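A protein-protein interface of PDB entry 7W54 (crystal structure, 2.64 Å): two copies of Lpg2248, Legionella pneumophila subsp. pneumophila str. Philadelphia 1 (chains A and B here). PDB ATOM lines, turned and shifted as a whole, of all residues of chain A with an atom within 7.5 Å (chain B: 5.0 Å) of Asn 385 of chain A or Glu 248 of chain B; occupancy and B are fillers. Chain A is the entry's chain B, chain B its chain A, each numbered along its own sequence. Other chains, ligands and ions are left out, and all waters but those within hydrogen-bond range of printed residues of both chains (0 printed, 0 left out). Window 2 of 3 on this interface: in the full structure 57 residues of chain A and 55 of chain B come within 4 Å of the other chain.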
ATOM      1  N   VAL A 382     -17.667   7.031  -9.412  1.00  0.00           N
ATOM      2  CA  VAL A 382     -17.378   5.853  -8.597  1.00  0.00           C
ATOM      3  C   VAL A 382     -18.049   6.033  -7.243  1.00  0.00           C
ATOM      4  O   VAL A 382     -18.009   7.121  -6.651  1.00  0.00           O
ATOM      5  CB  VAL A 382     -15.861   5.607  -8.468  1.00  0.00           C
ATOM      6  CG1 VAL A 382     -15.196   5.520  -9.841  1.00  0.00           C
ATOM      7  CG2 VAL A 382     -15.154   6.631  -7.554  1.00  0.00           C
ATOM      8  N   PHE A 383     -18.725   4.991  -6.770  1.00  0.00           N
ATOM      9  CA  PHE A 383     -19.521   5.146  -5.563  1.00  0.00           C
ATOM     10  C   PHE A 383     -18.618   5.350  -4.358  1.00  0.00           C
ATOM     11  O   PHE A 383     -17.802   4.484  -4.023  1.00  0.00           O
ATOM     12  CB  PHE A 383     -20.432   3.949  -5.326  1.00  0.00           C
ATOM     13  CG  PHE A 383     -21.372   4.157  -4.177  1.00  0.00           C
ATOM     14  CD1 PHE A 383     -22.121   5.320  -4.094  1.00  0.00           C
ATOM     15  CD2 PHE A 383     -21.469   3.229  -3.154  1.00  0.00           C
ATOM     16  CE1 PHE A 383     -22.979   5.539  -3.035  1.00  0.00           C
ATOM     17  CE2 PHE A 383     -22.328   3.441  -2.092  1.00  0.00           C
ATOM     18  CZ  PHE A 383     -23.081   4.599  -2.031  1.00  0.00           C
ATOM     19  N   ARG A 384     -18.759   6.506  -3.717  1.00  0.00           N
ATOM     20  CA  ARG A 384     -18.175   6.728  -2.405  1.00  0.00           C
ATOM     21  C   ARG A 384     -19.283   6.704  -1.363  1.00  0.00           C
ATOM     22  O   ARG A 384     -19.466   5.711  -0.653  1.00  0.00           O
ATOM     23  CB  ARG A 384     -17.432   8.063  -2.354  1.00  0.00           C
ATOM     24  CG  ARG A 384     -16.521   8.323  -3.537  1.00  0.00           C
ATOM     25  CD  ARG A 384     -16.348   9.812  -3.770  1.00  0.00           C
ATOM     26  NE  ARG A 384     -15.959  10.525  -2.555  1.00  0.00           N
ATOM     27  CZ  ARG A 384     -14.739  10.500  -2.025  1.00  0.00           C
ATOM     28  NH1 ARG A 384     -13.774   9.794  -2.601  1.00  0.00           N
ATOM     29  NH2 ARG A 384     -14.484  11.181  -0.916  1.00  0.00           N
ATOM     30  N   ASN A 385     -20.046   7.788  -1.298  1.00  0.00           N
ATOM     31  CA  ASN A 385     -21.020   8.021  -0.249  1.00  0.00           C
ATOM     32  C   ASN A 385     -22.416   8.148  -0.843  1.00  0.00           C
ATOM     33  O   ASN A 385     -22.589   8.492  -2.016  1.00  0.00           O
ATOM     34  CB  ASN A 385     -20.668   9.293   0.529  1.00  0.00           C
ATOM     35  CG  ASN A 385     -21.250   9.309   1.920  1.00  0.00           C
ATOM     36  OD1 ASN A 385     -21.331  10.359   2.555  1.00  0.00           O
ATOM     37  ND2 ASN A 385     -21.653   8.143   2.410  1.00  0.00           N
ATOM     38  N   GLY A 386     -23.419   7.870  -0.011  1.00  0.00           N
ATOM     39  CA  GLY A 386     -24.788   8.164  -0.392  1.00  0.00           C
ATOM     40  C   GLY A 386     -25.051   9.642  -0.575  1.00  0.00           C
ATOM     41  O   GLY A 386     -26.072  10.017  -1.162  1.00  0.00           O
ATOM     42  N   ASN A 387     -24.153  10.495  -0.076  1.00  0.00           N
ATOM     43  CA  ASN A 387     -24.242  11.924  -0.339  1.00  0.00           C
ATOM     44  C   ASN A 387     -23.877  12.270  -1.776  1.00  0.00           C
ATOM     45  O   ASN A 387     -24.251  13.348  -2.250  1.00  0.00           O
ATOM     46  CB  ASN A 387     -23.328  12.695   0.614  1.00  0.00           C
ATOM     47  CG  ASN A 387     -23.927  12.870   1.995  1.00  0.00           C
ATOM     48  OD1 ASN A 387     -25.000  13.452   2.151  1.00  0.00           O
ATOM     49  ND2 ASN A 387     -23.228  12.374   3.009  1.00  0.00           N
ATOM     50  N   TYR A 388     -23.163  11.382  -2.473  1.00  0.00           N
ATOM     51  CA  TYR A 388     -22.635  11.651  -3.812  1.00  0.00           C
ATOM     52  C   TYR A 388     -21.962  13.021  -3.860  1.00  0.00           C
ATOM     53  O   TYR A 388     -22.241  13.851  -4.728  1.00  0.00           O
ATOM     54  CB  TYR A 388     -23.734  11.535  -4.873  1.00  0.00           C
ATOM     55  CG  TYR A 388     -24.287  10.138  -5.039  1.00  0.00           C
ATOM     56  CD1 TYR A 388     -25.349   9.694  -4.260  1.00  0.00           C
ATOM     57  CD2 TYR A 388     -23.750   9.261  -5.975  1.00  0.00           C
ATOM     58  CE1 TYR A 388     -25.861   8.420  -4.405  1.00  0.00           C
ATOM     59  CE2 TYR A 388     -24.254   7.982  -6.128  1.00  0.00           C
ATOM     60  CZ  TYR A 388     -25.311   7.568  -5.339  1.00  0.00           C
ATOM     61  OH  TYR A 388     -25.824   6.300  -5.479  1.00  0.00           O
ATOM     62  N   ASN A 389     -21.067  13.254  -2.897  1.00  0.00           N
ATOM     63  CA  ASN A 389     -20.506  14.589  -2.716  1.00  0.00           C
ATOM     64  C   ASN A 389     -19.632  15.006  -3.893  1.00  0.00           C
ATOM     65  O   ASN A 389     -19.528  16.202  -4.189  1.00  0.00           O
ATOM     66  CB  ASN A 389     -19.716  14.654  -1.406  1.00  0.00           C
ATOM     67  CG  ASN A 389     -18.360  13.976  -1.499  1.00  0.00           C
ATOM     68  OD1 ASN A 389     -18.264  12.788  -1.812  1.00  0.00           O
ATOM     69  ND2 ASN A 389     -17.302  14.731  -1.215  1.00  0.00           N
ATOM     70  N   ARG A 390     -19.004  14.049  -4.575  1.00  0.00           N
ATOM     71  CA  ARG A 390     -18.185  14.401  -5.725  1.00  0.00           C
ATOM     72  C   ARG A 390     -19.014  14.520  -6.996  1.00  0.00           C
ATOM     73  O   ARG A 390     -18.695  15.345  -7.860  1.00  0.00           O
ATOM     74  CB  ARG A 390     -17.063  13.377  -5.908  1.00  0.00           C
ATOM     75  CG  ARG A 390     -16.128  13.295  -4.712  1.00  0.00           C
ATOM     76  CD  ARG A 390     -14.755  12.762  -5.085  1.00  0.00           C
ATOM     77  NE  ARG A 390     -13.765  13.069  -4.054  1.00  0.00           N
ATOM     78  CZ  ARG A 390     -12.574  12.488  -3.962  1.00  0.00           C
ATOM     79  NH1 ARG A 390     -12.216  11.558  -4.837  1.00  0.00           N
ATOM     80  NH2 ARG A 390     -11.739  12.833  -2.989  1.00  0.00           N
ATOM     81  N   PRO A 460     -26.105   2.066  -8.636  1.00  0.00           N
ATOM     82  CA  PRO A 460     -25.175   3.163  -8.322  1.00  0.00           C
ATOM     83  C   PRO A 460     -24.134   2.816  -7.273  1.00  0.00           C
ATOM     84  O   PRO A 460     -23.009   3.331  -7.335  1.00  0.00           O
ATOM     85  CB  PRO A 460     -26.113   4.274  -7.837  1.00  0.00           C
ATOM     86  CG  PRO A 460     -27.399   4.008  -8.540  1.00  0.00           C
ATOM     87  CD  PRO A 460     -27.510   2.512  -8.651  1.00  0.00           C
ATOM     88  N   LYS B   3     -21.124  -0.512   5.894  1.00  0.00           N
ATOM     89  CA  LYS B   3     -20.475  -0.188   4.633  1.00  0.00           C
ATOM     90  C   LYS B   3     -18.978   0.005   4.836  1.00  0.00           C
ATOM     91  O   LYS B   3     -18.527   0.469   5.889  1.00  0.00           O
ATOM     92  CB  LYS B   3     -21.082   1.076   4.014  1.00  0.00           C
ATOM     93  CG  LYS B   3     -22.597   1.152   4.133  1.00  0.00           C
ATOM     94  CD  LYS B   3     -23.125   2.518   3.728  1.00  0.00           C
ATOM     95  CE  LYS B   3     -23.315   2.608   2.222  1.00  0.00           C
ATOM     96  NZ  LYS B   3     -24.455   3.492   1.853  1.00  0.00           N
ATOM     97  N   GLU B 244     -24.254   2.740   8.174  1.00  0.00           N
ATOM     98  CA  GLU B 244     -24.691   3.618   7.084  1.00  0.00           C
ATOM     99  C   GLU B 244     -25.121   4.978   7.628  1.00  0.00           C
ATOM    100  O   GLU B 244     -24.740   6.037   7.096  1.00  0.00           O
ATOM    101  CB  GLU B 244     -25.830   2.971   6.287  1.00  0.00           C
ATOM    102  N   GLU B 245     -25.857   4.957   8.744  1.00  0.00           N
ATOM    103  CA  GLU B 245     -26.425   6.156   9.349  1.00  0.00           C
ATOM    104  C   GLU B 245     -25.390   7.256   9.562  1.00  0.00           C
ATOM    105  O   GLU B 245     -25.547   8.373   9.056  1.00  0.00           O
ATOM    106  CB  GLU B 245     -27.108   5.788  10.674  1.00  0.00           C
ATOM    107  N   ASP B 246     -24.315   6.964  10.304  1.00  0.00           N
ATOM    108  CA  ASP B 246     -23.314   8.002  10.543  1.00  0.00           C
ATOM    109  C   ASP B 246     -22.424   8.230   9.318  1.00  0.00           C
ATOM    110  O   ASP B 246     -21.920   9.350   9.127  1.00  0.00           O
ATOM    111  CB  ASP B 246     -22.491   7.682  11.810  1.00  0.00           C
ATOM    112  CG  ASP B 246     -22.040   6.233  11.890  1.00  0.00           C
ATOM    113  OD1 ASP B 246     -21.700   5.761  13.003  1.00  0.00           O
ATOM    114  OD2 ASP B 246     -21.990   5.577  10.839  1.00  0.00           O
ATOM    115  N   SER B 247     -22.259   7.201   8.468  1.00  0.00           N
ATOM    116  CA  SER B 247     -21.558   7.354   7.192  1.00  0.00           C
ATOM    117  C   SER B 247     -22.055   8.571   6.449  1.00  0.00           C
ATOM    118  O   SER B 247     -21.263   9.399   5.986  1.00  0.00           O
ATOM    119  CB  SER B 247     -21.760   6.134   6.294  1.00  0.00           C
ATOM    120  OG  SER B 247     -21.231   6.372   4.991  1.00  0.00           O
ATOM    121  N   GLU B 248     -23.377   8.696   6.321  1.00  0.00           N
ATOM    122  CA  GLU B 248     -23.893   9.797   5.522  1.00  0.00           C
ATOM    123  C   GLU B 248     -23.900  11.130   6.264  1.00  0.00           C
ATOM    124  O   GLU B 248     -23.893  12.183   5.616  1.00  0.00           O
ATOM    125  CB  GLU B 248     -25.294   9.461   5.016  1.00  0.00           C
ATOM    126  CG  GLU B 248     -25.273   8.550   3.796  1.00  0.00           C
ATOM    127  CD  GLU B 248     -25.636   7.116   4.134  1.00  0.00           C
ATOM    128  OE1 GLU B 248     -26.152   6.880   5.246  1.00  0.00           O
ATOM    129  OE2 GLU B 248     -25.392   6.222   3.297  1.00  0.00           O
ATOM    130  N   ARG B 249     -23.887  11.122   7.596  1.00  0.00           N
ATOM    131  CA  ARG B 249     -23.966  12.402   8.288  1.00  0.00           C
ATOM    132  C   ARG B 249     -22.603  13.055   8.460  1.00  0.00           C
ATOM    133  O   ARG B 249     -22.510  14.286   8.402  1.00  0.00           O
ATOM    134  CB  ARG B 249     -24.649  12.256   9.652  1.00  0.00           C
ATOM    135  CG  ARG B 249     -24.789  13.607  10.374  1.00  0.00           C
ATOM    136  CD  ARG B 249     -26.003  13.716  11.294  1.00  0.00           C
ATOM    137  NE  ARG B 249     -25.856  14.845  12.212  1.00  0.00           N
ATOM    138  CZ  ARG B 249     -26.035  14.778  13.528  1.00  0.00           C
ATOM    139  NH1 ARG B 249     -26.377  13.630  14.095  1.00  0.00           N
ATOM    140  NH2 ARG B 249     -25.871  15.862  14.278  1.00  0.00           N
ATOM    141  N   PHE B 250     -21.533  12.288   8.671  1.00  0.00           N
ATOM    142  CA  PHE B 250     -20.272  12.939   9.002  1.00  0.00           C
ATOM    143  C   PHE B 250     -19.127  12.666   8.034  1.00  0.00           C
ATOM    144  O   PHE B 250     -18.013  13.158   8.263  1.00  0.00           O
ATOM    145  CB  PHE B 250     -19.840  12.576  10.428  1.00  0.00           C
ATOM    146  CG  PHE B 250     -20.979  12.531  11.403  1.00  0.00           C
ATOM    147  CD1 PHE B 250     -21.296  13.641  12.173  1.00  0.00           C
ATOM    148  CD2 PHE B 250     -21.723  11.373  11.563  1.00  0.00           C
ATOM    149  CE1 PHE B 250     -22.341  13.599  13.074  1.00  0.00           C
ATOM    150  CE2 PHE B 250     -22.771  11.323  12.462  1.00  0.00           C
ATOM    151  CZ  PHE B 250     -23.078  12.439  13.222  1.00  0.00           C
ATOM    152  N   LEU B 251     -19.359  11.940   6.948  1.00  0.00           N
ATOM    153  CA  LEU B 251     -18.371  11.780   5.892  1.00  0.00           C
ATOM    154  C   LEU B 251     -18.958  12.261   4.575  1.00  0.00           C
ATOM    155  O   LEU B 251     -20.146  12.057   4.309  1.00  0.00           O
ATOM    156  CB  LEU B 251     -17.919  10.324   5.757  1.00  0.00           C
ATOM    157  CG  LEU B 251     -17.265   9.692   6.980  1.00  0.00           C
ATOM    158  CD1 LEU B 251     -16.916   8.232   6.721  1.00  0.00           C
ATOM    159  CD2 LEU B 251     -16.030  10.490   7.375  1.00  0.00           C
ATOM    160  N   ASP B 252     -18.123  12.912   3.766  1.00  0.00           N
ATOM    161  CA  ASP B 252     -18.495  13.328   2.414  1.00  0.00           C
ATOM    162  C   ASP B 252     -19.771  14.169   2.412  1.00  0.00           C
ATOM    163  O   ASP B 252     -20.698  13.929   1.641  1.00  0.00           O
ATOM    164  CB  ASP B 252     -18.645  12.115   1.493  1.00  0.00           C
ATOM    165  CG  ASP B 252     -17.325  11.410   1.229  1.00  0.00           C
ATOM    166  OD1 ASP B 252     -16.262  12.049   1.394  1.00  0.00           O
ATOM    167  OD2 ASP B 252     -17.349  10.219   0.849  1.00  0.00           O
ATOM    168  N   SER B 253     -19.818  15.166   3.296  1.00  0.00           N
ATOM    169  CA  SER B 253     -20.922  16.118   3.322  1.00  0.00           C
ATOM    170  C   SER B 253     -20.495  17.499   2.831  1.00  0.00           C
ATOM    171  O   SER B 253     -21.212  18.482   3.045  1.00  0.00           O
ATOM    172  CB  SER B 253     -21.527  16.204   4.726  1.00  0.00           C
ATOM    173  OG  SER B 253     -20.561  16.600   5.681  1.00  0.00           O
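The side-chain hydroxyl (OG) of Ser 247 of chain B lies within hydrogen-bond range of the side-chain amide nitrogen (ND2) of Asn 385 of chain A (3.2 Å). The backbone carbonyl oxygen of Glu 248 of chain B sits at hydrogen-bond distance from the side-chain amide nitrogen of Asn 387 of chain A, at 2.7 Å. The backbone carbonyl oxygen (O) of Leu 251 of chain B sits close to the side-chain amide oxygen (OD1) of Asn 385 of chain A (2.7 Å). The side-chain amide nitrogen (ND2) of Asn 387 of chain A is in hydrogen-bond range of the backbone carbonyl oxygen (O) of Leu 251 of chain B (3.4 Å). The side-chain carboxylate (OD1) of Asp 252 of chain B is in salt-bridge range of the guanidinium group (NH2) of Arg 384 of chain A (3.0 Å). The backbone carbonyl oxygen of Asp 252 of chain B sits close to the side-chain amide nitrogen of Asn 387 of chain A, at 3.3 Å.
The side-chain carboxylate of Glu 248 of chain B is in salt-bridge range of the side-chain amino group of Lys 3 of chain B (3.2 Å). The side-chain carboxylate (OE1) of Glu 248 of chain B lies close to the backbone carbonyl oxygen (O) of Glu 244 of chain B (2.5 Å). OD1 of Asn 389 of chain A sits at hydrogen-bond distance from NE of Arg 384 of chain A. The side-chain amide nitrogen (ND2) of Asn 387 of chain A is in hydrogen-bond range of the side-chain amide oxygen (OD1) of Asn 385 of chain A (2.8 Å).
Among the printed residues, merely in contact across the chains: Asn 389 of chain A with Asp 252 of chain B, Asn 385 of chain A with Asp 252 of chain B and Asn 385 of chain A with Glu 248 of chain B.
Of the printed residues of chain B, Arg 384 of chain A touches Asp 252. Of the printed residues of chain B, Asn 385 of chain A touches Ser 247 (3.2 Å), Glu 248 (3.9 Å), Leu 251 (2.7 Å) and Asp 252 (3.4 Å). Of the printed residues of chain B, Asn 387 of chain A touches Glu 248, Leu 251 and Asp 252. Printed residues of chain B within 4 Å of Asn 389 of chain A: Asp 252. Lys 3 of chain B touches none of the printed residues of chain A. Glu 248 of chain B touches two residues of chain A. Of the printed residues of chain A, Asp 252 of chain B touches Arg 384 (3.0 Å), Asn 385 (3.4 Å), Asn 387 (3.1 Å) and Asn 389 (3.3 Å). The nearest residue of chain A that does not touch Glu 248 of chain B is Gly 386 of chain A (4.2 Å). The nearest printed residue of chain A that does not touch Asp 252 of chain B is Tyr 388 of chain A (5.4 Å).
Printed residues of chain B that touch a printed residue of chain A: Ser 247, Glu 248, Leu 251 and Asp 252.
No position is printed for both chains.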
